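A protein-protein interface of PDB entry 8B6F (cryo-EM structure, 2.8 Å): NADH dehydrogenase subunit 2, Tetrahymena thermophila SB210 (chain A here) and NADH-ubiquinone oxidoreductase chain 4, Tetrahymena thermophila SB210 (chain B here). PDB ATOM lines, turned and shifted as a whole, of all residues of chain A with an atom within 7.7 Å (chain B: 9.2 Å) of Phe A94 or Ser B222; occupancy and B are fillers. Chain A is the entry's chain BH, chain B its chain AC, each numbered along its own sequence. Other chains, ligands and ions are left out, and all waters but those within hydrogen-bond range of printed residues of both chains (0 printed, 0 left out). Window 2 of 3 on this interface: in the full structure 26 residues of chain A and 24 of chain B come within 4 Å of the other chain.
The side-chain hydroxyl of Ser B222 is in hydrogen-bond range of the backbone carbonyl oxygen of Leu A90.
OG of Ser B222 is in hydrogen-bond range of N of Phe A94 (3.4 Å).
The backbone carbonyl oxygen (O) of Leu B214 lies within hydrogen-bond range of the side-chain hydroxyl (OG) of Ser B218.
The backbone carbonyl oxygen of Ser B218 sits at hydrogen-bond distance from the side-chain hydroxyl of Ser B222 (3.0 Å).
The backbone carbonyl oxygen (O) of Ile A89 is in hydrogen-bond range of the side-chain hydroxyl (OG) of Ser A93 (3.1 Å).
Among the printed residues, pairs that only touch across the chains: Phe A86 with Ser B218 (3.3 Å), Phe A86 with Leu B214 (3.4 Å), Ser A93 with Ser B218 (3.5 Å), Ser A93 with Ser B222 (3.5 Å), Ile A89 with Leu B214 (3.5 Å), Ile A89 with Ser B218 (3.5 Å), Leu A90 with Ser B218 (3.6 Å) and Ile A101 with Ile B215 (3.8 Å).
Of the printed residues of chain B, Leu A90 touches Ser B218 and Ser B222.
Of the printed residues of chain B, Ser A93 touches Ser B218 and Ser B222.
Printed residues of chain B within 4 Å of Phe A94: Ser B222 (3.4 Å).
Ser B222 touches just these residues of chain A: Leu A90, Ser A93 and Phe A94.
Ile B245 touches none of the printed residues of chain A.
The nearest residue of chain B that does not touch Phe A94 is Ser B218 (5.6 Å).
Printed residues of chain B that touch a printed residue of chain A: Leu B214, Ile B215, Ser B218 and Ser B222.
Hydrophobic or aromatic side chains of chain A within 4 Å of the printed part of chain B: Phe A86, Ile A89, Leu A90, Phe A94 and Ile A101.
Along chain A the printed residues that touch a printed residue of chain B span positions 86 to 101.
Among the printed residues, 10 pairs touch across the chains.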
ATOM      1  N   ASN A  11     -34.547   1.331  12.647  1.00  0.00           N
ATOM      2  CA  ASN A  11     -35.200   0.422  13.574  1.00  0.00           C
ATOM      3  C   ASN A  11     -34.664   0.562  14.992  1.00  0.00           C
ATOM      4  O   ASN A  11     -34.988  -0.266  15.849  1.00  0.00           O
ATOM      5  CB  ASN A  11     -35.035  -1.022  13.101  1.00  0.00           C
ATOM      6  CG  ASN A  11     -35.611  -1.252  11.721  1.00  0.00           C
ATOM      7  OD1 ASN A  11     -36.505  -0.533  11.280  1.00  0.00           O
ATOM      8  ND2 ASN A  11     -35.101  -2.264  11.030  1.00  0.00           N
ATOM      9  N   ASP A  12     -33.846   1.578  15.254  1.00  0.00           N
ATOM     10  CA  ASP A  12     -33.266   1.811  16.568  1.00  0.00           C
ATOM     11  C   ASP A  12     -33.792   3.121  17.131  1.00  0.00           C
ATOM     12  O   ASP A  12     -33.874   4.126  16.419  1.00  0.00           O
ATOM     13  CB  ASP A  12     -31.737   1.853  16.499  1.00  0.00           C
ATOM     14  CG  ASP A  12     -31.143   0.576  15.941  1.00  0.00           C
ATOM     15  OD1 ASP A  12     -31.759  -0.495  16.122  1.00  0.00           O
ATOM     16  OD2 ASP A  12     -30.062   0.640  15.320  1.00  0.00           O
ATOM     17  N   LEU A  13     -34.149   3.103  18.411  1.00  0.00           N
ATOM     18  CA  LEU A  13     -34.620   4.285  19.122  1.00  0.00           C
ATOM     19  C   LEU A  13     -33.445   4.849  19.909  1.00  0.00           C
ATOM     20  O   LEU A  13     -33.013   4.256  20.903  1.00  0.00           O
ATOM     21  CB  LEU A  13     -35.790   3.936  20.039  1.00  0.00           C
ATOM     22  CG  LEU A  13     -36.452   5.098  20.782  1.00  0.00           C
ATOM     23  CD1 LEU A  13     -37.122   6.050  19.807  1.00  0.00           C
ATOM     24  CD2 LEU A  13     -37.453   4.575  21.795  1.00  0.00           C
ATOM     25  N   ASN A  14     -32.927   5.995  19.464  1.00  0.00           N
ATOM     26  CA  ASN A  14     -31.723   6.545  20.076  1.00  0.00           C
ATOM     27  C   ASN A  14     -31.966   6.937  21.527  1.00  0.00           C
ATOM     28  O   ASN A  14     -31.095   6.746  22.383  1.00  0.00           O
ATOM     29  CB  ASN A  14     -31.235   7.748  19.271  1.00  0.00           C
ATOM     30  CG  ASN A  14     -29.816   8.138  19.615  1.00  0.00           C
ATOM     31  OD1 ASN A  14     -29.163   7.489  20.430  1.00  0.00           O
ATOM     32  ND2 ASN A  14     -29.326   9.198  18.987  1.00  0.00           N
ATOM     33  N   TYR A  16     -33.178   5.753  24.146  1.00  0.00           N
ATOM     34  CA  TYR A  16     -33.508   4.574  24.935  1.00  0.00           C
ATOM     35  C   TYR A  16     -32.500   4.300  26.036  1.00  0.00           C
ATOM     36  O   TYR A  16     -32.887   3.885  27.129  1.00  0.00           O
ATOM     37  CB  TYR A  16     -33.617   3.342  24.024  1.00  0.00           C
ATOM     38  CG  TYR A  16     -34.213   2.136  24.712  1.00  0.00           C
ATOM     39  CD1 TYR A  16     -33.407   1.221  25.376  1.00  0.00           C
ATOM     40  CD2 TYR A  16     -35.582   1.914  24.700  1.00  0.00           C
ATOM     41  CE1 TYR A  16     -33.947   0.119  26.009  1.00  0.00           C
ATOM     42  CE2 TYR A  16     -36.134   0.816  25.330  1.00  0.00           C
ATOM     43  CZ  TYR A  16     -35.311  -0.077  25.982  1.00  0.00           C
ATOM     44  OH  TYR A  16     -35.856  -1.172  26.611  1.00  0.00           O
ATOM     45  N   PHE A  86     -31.011  -6.004  34.705  1.00  0.00           N
ATOM     46  CA  PHE A  86     -31.267  -6.775  33.495  1.00  0.00           C
ATOM     47  C   PHE A  86     -31.393  -5.871  32.279  1.00  0.00           C
ATOM     48  O   PHE A  86     -30.867  -6.183  31.205  1.00  0.00           O
ATOM     49  CB  PHE A  86     -32.536  -7.612  33.681  1.00  0.00           C
ATOM     50  CG  PHE A  86     -32.791  -8.613  32.580  1.00  0.00           C
ATOM     51  CD1 PHE A  86     -31.804  -8.953  31.667  1.00  0.00           C
ATOM     52  CD2 PHE A  86     -34.031  -9.215  32.465  1.00  0.00           C
ATOM     53  CE1 PHE A  86     -32.052  -9.871  30.665  1.00  0.00           C
ATOM     54  CE2 PHE A  86     -34.284 -10.133  31.465  1.00  0.00           C
ATOM     55  CZ  PHE A  86     -33.294 -10.462  30.565  1.00  0.00           C
ATOM     56  N   LEU A  87     -32.074  -4.735  32.429  1.00  0.00           N
ATOM     57  CA  LEU A  87     -32.215  -3.813  31.310  1.00  0.00           C
ATOM     58  C   LEU A  87     -30.894  -3.148  30.952  1.00  0.00           C
ATOM     59  O   LEU A  87     -30.641  -2.875  29.774  1.00  0.00           O
ATOM     60  CB  LEU A  87     -33.279  -2.770  31.629  1.00  0.00           C
ATOM     61  CG  LEU A  87     -34.712  -3.306  31.607  1.00  0.00           C
ATOM     62  CD1 LEU A  87     -35.675  -2.294  32.184  1.00  0.00           C
ATOM     63  CD2 LEU A  87     -35.132  -3.686  30.195  1.00  0.00           C
ATOM     64  N   ALA A  88     -30.048  -2.864  31.944  1.00  0.00           N
ATOM     65  CA  ALA A  88     -28.717  -2.356  31.634  1.00  0.00           C
ATOM     66  C   ALA A  88     -27.924  -3.368  30.818  1.00  0.00           C
ATOM     67  O   ALA A  88     -27.265  -3.007  29.838  1.00  0.00           O
ATOM     68  CB  ALA A  88     -27.974  -2.011  32.924  1.00  0.00           C
ATOM     69  N   ILE A  89     -27.971  -4.641  31.213  1.00  0.00           N
ATOM     70  CA  ILE A  89     -27.258  -5.675  30.469  1.00  0.00           C
ATOM     71  C   ILE A  89     -27.852  -5.828  29.076  1.00  0.00           C
ATOM     72  O   ILE A  89     -27.127  -6.034  28.096  1.00  0.00           O
ATOM     73  CB  ILE A  89     -27.272  -7.002  31.248  1.00  0.00           C
ATOM     74  CG1 ILE A  89     -26.440  -6.868  32.525  1.00  0.00           C
ATOM     75  CG2 ILE A  89     -26.717  -8.134  30.390  1.00  0.00           C
ATOM     76  CD1 ILE A  89     -26.550  -8.051  33.467  1.00  0.00           C
ATOM     77  N   LEU A  90     -29.179  -5.740  28.963  1.00  0.00           N
ATOM     78  CA  LEU A  90     -29.819  -5.843  27.656  1.00  0.00           C
ATOM     79  C   LEU A  90     -29.381  -4.712  26.738  1.00  0.00           C
ATOM     80  O   LEU A  90     -29.109  -4.935  25.553  1.00  0.00           O
ATOM     81  CB  LEU A  90     -31.338  -5.837  27.813  1.00  0.00           C
ATOM     82  CG  LEU A  90     -31.982  -7.156  28.232  1.00  0.00           C
ATOM     83  CD1 LEU A  90     -33.362  -6.922  28.813  1.00  0.00           C
ATOM     84  CD2 LEU A  90     -32.064  -8.082  27.039  1.00  0.00           C
ATOM     85  N   TYR A  91     -29.321  -3.487  27.260  1.00  0.00           N
ATOM     86  CA  TYR A  91     -28.879  -2.367  26.439  1.00  0.00           C
ATOM     87  C   TYR A  91     -27.406  -2.495  26.073  1.00  0.00           C
ATOM     88  O   TYR A  91     -27.007  -2.153  24.954  1.00  0.00           O
ATOM     89  CB  TYR A  91     -29.144  -1.048  27.162  1.00  0.00           C
ATOM     90  CG  TYR A  91     -28.860   0.163  26.307  1.00  0.00           C
ATOM     91  CD1 TYR A  91     -29.699   0.508  25.258  1.00  0.00           C
ATOM     92  CD2 TYR A  91     -27.756   0.963  26.553  1.00  0.00           C
ATOM     93  CE1 TYR A  91     -29.444   1.612  24.475  1.00  0.00           C
ATOM     94  CE2 TYR A  91     -27.491   2.067  25.777  1.00  0.00           C
ATOM     95  CZ  TYR A  91     -28.338   2.389  24.740  1.00  0.00           C
ATOM     96  OH  TYR A  91     -28.075   3.491  23.964  1.00  0.00           O
ATOM     97  N   SER A  92     -26.581  -2.993  26.995  1.00  0.00           N
ATOM     98  CA  SER A  92     -25.179  -3.226  26.667  1.00  0.00           C
ATOM     99  C   SER A  92     -25.047  -4.240  25.540  1.00  0.00           C
ATOM    100  O   SER A  92     -24.242  -4.056  24.620  1.00  0.00           O
ATOM    101  CB  SER A  92     -24.422  -3.704  27.906  1.00  0.00           C
ATOM    102  OG  SER A  92     -24.522  -2.761  28.959  1.00  0.00           O
ATOM    103  N   SER A  93     -25.826  -5.321  25.595  1.00  0.00           N
ATOM    104  CA  SER A  93     -25.804  -6.296  24.511  1.00  0.00           C
ATOM    105  C   SER A  93     -26.284  -5.670  23.210  1.00  0.00           C
ATOM    106  O   SER A  93     -25.724  -5.931  22.141  1.00  0.00           O
ATOM    107  CB  SER A  93     -26.664  -7.506  24.876  1.00  0.00           C
ATOM    108  OG  SER A  93     -26.158  -8.166  26.021  1.00  0.00           O
ATOM    109  N   PHE A  94     -27.326  -4.840  23.284  1.00  0.00           N
ATOM    110  CA  PHE A  94     -27.827  -4.165  22.093  1.00  0.00           C
ATOM    111  C   PHE A  94     -26.756  -3.275  21.479  1.00  0.00           C
ATOM    112  O   PHE A  94     -26.622  -3.207  20.251  1.00  0.00           O
ATOM    113  CB  PHE A  94     -29.071  -3.351  22.450  1.00  0.00           C
ATOM    114  CG  PHE A  94     -29.749  -2.726  21.269  1.00  0.00           C
ATOM    115  CD1 PHE A  94     -30.594  -3.473  20.470  1.00  0.00           C
ATOM    116  CD2 PHE A  94     -29.560  -1.389  20.969  1.00  0.00           C
ATOM    117  CE1 PHE A  94     -31.226  -2.904  19.387  1.00  0.00           C
ATOM    118  CE2 PHE A  94     -30.191  -0.813  19.887  1.00  0.00           C
ATOM    119  CZ  PHE A  94     -31.025  -1.572  19.094  1.00  0.00           C
ATOM    120  N   LYS A  95     -25.981  -2.589  22.317  1.00  0.00           N
ATOM    121  CA  LYS A  95     -24.878  -1.758  21.854  1.00  0.00           C
ATOM    122  C   LYS A  95     -23.624  -2.565  21.552  1.00  0.00           C
ATOM    123  O   LYS A  95     -22.630  -1.986  21.102  1.00  0.00           O
ATOM    124  CB  LYS A  95     -24.559  -0.681  22.893  1.00  0.00           C
ATOM    125  CG  LYS A  95     -25.746   0.202  23.253  1.00  0.00           C
ATOM    126  CD  LYS A  95     -26.127   1.149  22.124  1.00  0.00           C
ATOM    127  CE  LYS A  95     -25.142   2.298  22.013  1.00  0.00           C
ATOM    128  NZ  LYS A  95     -25.547   3.288  20.981  1.00  0.00           N
ATOM    129  N   SER A  96     -23.642  -3.874  21.800  1.00  0.00           N
ATOM    130  CA  SER A  96     -22.534  -4.758  21.454  1.00  0.00           C
ATOM    131  C   SER A  96     -21.277  -4.412  22.252  1.00  0.00           C
ATOM    132  O   SER A  96     -20.211  -4.137  21.701  1.00  0.00           O
ATOM    133  CB  SER A  96     -22.273  -4.676  19.951  1.00  0.00           C
ATOM    134  OG  SER A  96     -23.490  -4.862  19.257  1.00  0.00           O
ATOM    135  N   GLN A  97     -21.421  -4.444  23.574  1.00  0.00           N
ATOM    136  CA  GLN A  97     -20.326  -4.162  24.499  1.00  0.00           C
ATOM    137  C   GLN A  97     -20.122  -5.391  25.373  1.00  0.00           C
ATOM    138  O   GLN A  97     -20.641  -5.474  26.487  1.00  0.00           O
ATOM    139  CB  GLN A  97     -20.638  -2.928  25.328  1.00  0.00           C
ATOM    140  CG  GLN A  97     -21.104  -1.746  24.501  1.00  0.00           C
ATOM    141  CD  GLN A  97     -20.129  -1.395  23.403  1.00  0.00           C
ATOM    142  OE1 GLN A  97     -18.916  -1.399  23.607  1.00  0.00           O
ATOM    143  NE2 GLN A  97     -20.654  -1.100  22.224  1.00  0.00           N
ATOM    144  N   ILE A 101     -20.205  -5.670  29.421  1.00  0.00           N
ATOM    145  CA  ILE A 101     -21.050  -6.671  30.061  1.00  0.00           C
ATOM    146  C   ILE A 101     -20.235  -7.476  31.061  1.00  0.00           C
ATOM    147  O   ILE A 101     -20.681  -7.728  32.183  1.00  0.00           O
ATOM    148  CB  ILE A 101     -21.714  -7.575  29.005  1.00  0.00           C
ATOM    149  CG1 ILE A 101     -22.808  -6.806  28.264  1.00  0.00           C
ATOM    150  CG2 ILE A 101     -22.299  -8.828  29.653  1.00  0.00           C
ATOM    151  CD1 ILE A 101     -23.342  -7.520  27.043  1.00  0.00           C
ATOM    152  N   LEU B 214     -28.486 -15.024  32.138  1.00  0.00           N
ATOM    153  CA  LEU B 214     -29.045 -13.715  31.821  1.00  0.00           C
ATOM    154  C   LEU B 214     -28.272 -13.043  30.696  1.00  0.00           C
ATOM    155  O   LEU B 214     -28.866 -12.419  29.809  1.00  0.00           O
ATOM    156  CB  LEU B 214     -29.051 -12.838  33.076  1.00  0.00           C
ATOM    157  CG  LEU B 214     -29.727 -11.463  33.024  1.00  0.00           C
ATOM    158  CD1 LEU B 214     -30.068 -10.999  34.424  1.00  0.00           C
ATOM    159  CD2 LEU B 214     -28.844 -10.413  32.350  1.00  0.00           C
ATOM    160  N   ILE B 215     -26.944 -13.154  30.714  1.00  0.00           N
ATOM    161  CA  ILE B 215     -26.141 -12.592  29.632  1.00  0.00           C
ATOM    162  C   ILE B 215     -26.476 -13.276  28.317  1.00  0.00           C
ATOM    163  O   ILE B 215     -26.611 -12.623  27.276  1.00  0.00           O
ATOM    164  CB  ILE B 215     -24.648 -12.748  29.963  1.00  0.00           C
ATOM    165  CG1 ILE B 215     -24.308 -12.016  31.252  1.00  0.00           C
ATOM    166  CG2 ILE B 215     -23.792 -12.197  28.831  1.00  0.00           C
ATOM    167  CD1 ILE B 215     -23.042 -12.529  31.858  1.00  0.00           C
ATOM    168  N   ALA B 216     -26.613 -14.603  28.339  1.00  0.00           N
ATOM    169  CA  ALA B 216     -26.966 -15.327  27.124  1.00  0.00           C
ATOM    170  C   ALA B 216     -28.328 -14.891  26.604  1.00  0.00           C
ATOM    171  O   ALA B 216     -28.506 -14.686  25.398  1.00  0.00           O
ATOM    172  CB  ALA B 216     -26.945 -16.833  27.387  1.00  0.00           C
ATOM    173  N   ILE B 217     -29.302 -14.743  27.502  1.00  0.00           N
ATOM    174  CA  ILE B 217     -30.636 -14.319  27.091  1.00  0.00           C
ATOM    175  C   ILE B 217     -30.588 -12.910  26.525  1.00  0.00           C
ATOM    176  O   ILE B 217     -31.280 -12.590  25.553  1.00  0.00           O
ATOM    177  CB  ILE B 217     -31.612 -14.418  28.277  1.00  0.00           C
ATOM    178  CG1 ILE B 217     -31.802 -15.878  28.680  1.00  0.00           C
ATOM    179  CG2 ILE B 217     -32.951 -13.762  27.940  1.00  0.00           C
ATOM    180  CD1 ILE B 217     -32.540 -16.705  27.672  1.00  0.00           C
ATOM    181  N   SER B 218     -29.773 -12.044  27.126  1.00  0.00           N
ATOM    182  CA  SER B 218     -29.618 -10.695  26.599  1.00  0.00           C
ATOM    183  C   SER B 218     -29.002 -10.719  25.207  1.00  0.00           C
ATOM    184  O   SER B 218     -29.412  -9.956  24.326  1.00  0.00           O
ATOM    185  CB  SER B 218     -28.767  -9.861  27.553  1.00  0.00           C
ATOM    186  OG  SER B 218     -29.320  -9.884  28.857  1.00  0.00           O
ATOM    187  N   TYR B 219     -28.008 -11.581  24.991  1.00  0.00           N
ATOM    188  CA  TYR B 219     -27.436 -11.720  23.657  1.00  0.00           C
ATOM    189  C   TYR B 219     -28.501 -12.134  22.650  1.00  0.00           C
ATOM    190  O   TYR B 219     -28.581 -11.581  21.548  1.00  0.00           O
ATOM    191  CB  TYR B 219     -26.300 -12.745  23.684  1.00  0.00           C
ATOM    192  CG  TYR B 219     -24.916 -12.143  23.727  1.00  0.00           C
ATOM    193  CD1 TYR B 219     -24.311 -11.831  24.938  1.00  0.00           C
ATOM    194  CD2 TYR B 219     -24.211 -11.896  22.560  1.00  0.00           C
ATOM    195  CE1 TYR B 219     -23.044 -11.284  24.984  1.00  0.00           C
ATOM    196  CE2 TYR B 219     -22.943 -11.350  22.594  1.00  0.00           C
ATOM    197  CZ  TYR B 219     -22.365 -11.046  23.810  1.00  0.00           C
ATOM    198  OH  TYR B 219     -21.103 -10.502  23.850  1.00  0.00           O
ATOM    199  N   ILE B 220     -29.331 -13.113  23.013  1.00  0.00           N
ATOM    200  CA  ILE B 220     -30.343 -13.611  22.086  1.00  0.00           C
ATOM    201  C   ILE B 220     -31.390 -12.538  21.809  1.00  0.00           C
ATOM    202  O   ILE B 220     -31.776 -12.307  20.657  1.00  0.00           O
ATOM    203  CB  ILE B 220     -30.981 -14.900  22.637  1.00  0.00           C
ATOM    204  CG1 ILE B 220     -29.959 -16.041  22.622  1.00  0.00           C
ATOM    205  CG2 ILE B 220     -32.210 -15.291  21.822  1.00  0.00           C
ATOM    206  CD1 ILE B 220     -30.418 -17.300  23.331  1.00  0.00           C
ATOM    207  N   ILE B 221     -31.870 -11.870  22.859  1.00  0.00           N
ATOM    208  CA  ILE B 221     -32.968 -10.922  22.697  1.00  0.00           C
ATOM    209  C   ILE B 221     -32.500  -9.671  21.965  1.00  0.00           C
ATOM    210  O   ILE B 221     -33.183  -9.167  21.066  1.00  0.00           O
ATOM    211  CB  ILE B 221     -33.587 -10.582  24.065  1.00  0.00           C
ATOM    212  CG1 ILE B 221     -34.435 -11.758  24.557  1.00  0.00           C
ATOM    213  CG2 ILE B 221     -34.423  -9.305  23.987  1.00  0.00           C
ATOM    214  CD1 ILE B 221     -34.959 -11.604  25.967  1.00  0.00           C
ATOM    215  N   SER B 222     -31.343  -9.133  22.350  1.00  0.00           N
ATOM    216  CA  SER B 222     -30.857  -7.921  21.700  1.00  0.00           C
ATOM    217  C   SER B 222     -30.575  -8.159  20.224  1.00  0.00           C
ATOM    218  O   SER B 222     -30.908  -7.320  19.379  1.00  0.00           O
ATOM    219  CB  SER B 222     -29.604  -7.412  22.410  1.00  0.00           C
ATOM    220  OG  SER B 222     -29.906  -7.029  23.738  1.00  0.00           O
ATOM    221  N   ILE B 223     -29.959  -9.293  19.894  1.00  0.00           N
ATOM    222  CA  ILE B 223     -29.671  -9.607  18.497  1.00  0.00           C
ATOM    223  C   ILE B 223     -30.962  -9.925  17.754  1.00  0.00           C
ATOM    224  O   ILE B 223     -31.297  -9.289  16.749  1.00  0.00           O
ATOM    225  CB  ILE B 223     -28.664 -10.768  18.406  1.00  0.00           C
ATOM    226  CG1 ILE B 223     -27.351 -10.380  19.091  1.00  0.00           C
ATOM    227  CG2 ILE B 223     -28.411 -11.145  16.953  1.00  0.00           C
ATOM    228  CD1 ILE B 223     -26.385 -11.531  19.271  1.00  0.00           C
ATOM    229  N   THR B 224     -31.704 -10.911  18.243  1.00  0.00           N
ATOM    230  CA  THR B 224     -33.012 -11.264  17.701  1.00  0.00           C
ATOM    231  C   THR B 224     -34.070 -10.639  18.594  1.00  0.00           C
ATOM    232  O   THR B 224     -34.232 -11.041  19.751  1.00  0.00           O
ATOM    233  CB  THR B 224     -33.195 -12.778  17.631  1.00  0.00           C
ATOM    234  OG1 THR B 224     -33.245 -13.317  18.958  1.00  0.00           O
ATOM    235  CG2 THR B 224     -32.056 -13.414  16.872  1.00  0.00           C
ATOM    236  N   ASN B 225     -34.804  -9.668  18.054  1.00  0.00           N
ATOM    237  CA  ASN B 225     -35.836  -9.000  18.833  1.00  0.00           C
ATOM    238  C   ASN B 225     -37.010  -9.916  19.144  1.00  0.00           C
ATOM    239  O   ASN B 225     -37.873  -9.542  19.944  1.00  0.00           O
ATOM    240  CB  ASN B 225     -36.318  -7.757  18.085  1.00  0.00           C
ATOM    241  CG  ASN B 225     -37.233  -6.895  18.922  1.00  0.00           C
ATOM    242  OD1 ASN B 225     -37.214  -6.963  20.149  1.00  0.00           O
ATOM    243  ND2 ASN B 225     -38.036  -6.073  18.263  1.00  0.00           N
ATOM    244  N   THR B 226     -37.055 -11.104  18.548  1.00  0.00           N
ATOM    245  CA  THR B 226     -38.161 -12.023  18.755  1.00  0.00           C
ATOM    246  C   THR B 226     -38.164 -12.560  20.183  1.00  0.00           C
ATOM    247  O   THR B 226     -37.165 -12.506  20.905  1.00  0.00           O
ATOM    248  CB  THR B 226     -38.074 -13.197  17.776  1.00  0.00           C
ATOM    249  OG1 THR B 226     -36.909 -13.983  18.060  1.00  0.00           O
ATOM    250  CG2 THR B 226     -38.017 -12.698  16.348  1.00  0.00           C
ATOM    251  N   TYR B 227     -39.321 -13.083  20.581  1.00  0.00           N
ATOM    252  CA  TYR B 227     -39.465 -13.763  21.858  1.00  0.00           C
ATOM    253  C   TYR B 227     -40.303 -15.028  21.766  1.00  0.00           C
ATOM    254  O   TYR B 227     -40.536 -15.664  22.798  1.00  0.00           O
ATOM    255  CB  TYR B 227     -40.091 -12.821  22.900  1.00  0.00           C
ATOM    256  CG  TYR B 227     -41.506 -12.407  22.567  1.00  0.00           C
ATOM    257  CD1 TYR B 227     -42.585 -13.194  22.945  1.00  0.00           C
ATOM    258  CD2 TYR B 227     -41.762 -11.232  21.877  1.00  0.00           C
ATOM    259  CE1 TYR B 227     -43.878 -12.826  22.647  1.00  0.00           C
ATOM    260  CE2 TYR B 227     -43.053 -10.853  21.572  1.00  0.00           C
ATOM    261  CZ  TYR B 227     -44.107 -11.656  21.960  1.00  0.00           C
ATOM    262  OH  TYR B 227     -45.396 -11.287  21.662  1.00  0.00           O
ATOM    263  N   PHE B 235     -33.441 -16.954  11.927  1.00  0.00           N
ATOM    264  CA  PHE B 235     -32.268 -16.149  12.234  1.00  0.00           C
ATOM    265  C   PHE B 235     -31.125 -17.075  12.615  1.00  0.00           C
ATOM    266  O   PHE B 235     -31.300 -17.966  13.451  1.00  0.00           O
ATOM    267  CB  PHE B 235     -32.554 -15.164  13.369  1.00  0.00           C
ATOM    268  CG  PHE B 235     -31.482 -14.135  13.560  1.00  0.00           C
ATOM    269  CD1 PHE B 235     -30.368 -14.409  14.335  1.00  0.00           C
ATOM    270  CD2 PHE B 235     -31.587 -12.893  12.960  1.00  0.00           C
ATOM    271  CE1 PHE B 235     -29.384 -13.462  14.510  1.00  0.00           C
ATOM    272  CE2 PHE B 235     -30.607 -11.941  13.132  1.00  0.00           C
ATOM    273  CZ  PHE B 235     -29.503 -12.227  13.908  1.00  0.00           C
ATOM    274  N   PHE B 237     -27.201 -17.332  14.064  1.00  0.00           N
ATOM    275  CA  PHE B 237     -26.126 -16.656  14.773  1.00  0.00           C
ATOM    276  C   PHE B 237     -24.780 -17.005  14.153  1.00  0.00           C
ATOM    277  O   PHE B 237     -24.528 -18.155  13.788  1.00  0.00           O
ATOM    278  CB  PHE B 237     -26.130 -17.049  16.251  1.00  0.00           C
ATOM    279  CG  PHE B 237     -27.313 -16.531  17.013  1.00  0.00           C
ATOM    280  CD1 PHE B 237     -28.496 -17.250  17.056  1.00  0.00           C
ATOM    281  CD2 PHE B 237     -27.240 -15.327  17.693  1.00  0.00           C
ATOM    282  CE1 PHE B 237     -29.587 -16.775  17.758  1.00  0.00           C
ATOM    283  CE2 PHE B 237     -28.326 -14.846  18.398  1.00  0.00           C
ATOM    284  CZ  PHE B 237     -29.502 -15.571  18.430  1.00  0.00           C
ATOM    285  N   GLU B 241     -20.928 -15.563  17.944  1.00  0.00           N
ATOM    286  CA  GLU B 241     -22.109 -15.409  18.786  1.00  0.00           C
ATOM    287  C   GLU B 241     -22.592 -16.759  19.296  1.00  0.00           C
ATOM    288  O   GLU B 241     -22.954 -16.898  20.469  1.00  0.00           O
ATOM    289  CB  GLU B 241     -23.219 -14.703  18.009  1.00  0.00           C
ATOM    290  CG  GLU B 241     -22.828 -13.330  17.494  1.00  0.00           C
ATOM    291  CD  GLU B 241     -23.870 -12.743  16.565  1.00  0.00           C
ATOM    292  OE1 GLU B 241     -24.951 -13.350  16.422  1.00  0.00           O
ATOM    293  OE2 GLU B 241     -23.608 -11.677  15.971  1.00  0.00           O
ATOM    294  N   ILE B 245     -22.792 -17.979  23.176  1.00  0.00           N
ATOM    295  CA  ILE B 245     -24.080 -18.346  23.759  1.00  0.00           C
ATOM    296  C   ILE B 245     -24.007 -19.731  24.389  1.00  0.00           C
ATOM    297  O   ILE B 245     -24.478 -19.945  25.510  1.00  0.00           O
ATOM    298  CB  ILE B 245     -25.191 -18.261  22.696  1.00  0.00           C
ATOM    299  CG1 ILE B 245     -25.482 -16.795  22.362  1.00  0.00           C
ATOM    300  CG2 ILE B 245     -26.462 -18.964  23.173  1.00  0.00           C
ATOM    301  CD1 ILE B 245     -26.409 -16.597  21.186  1.00  0.00           C
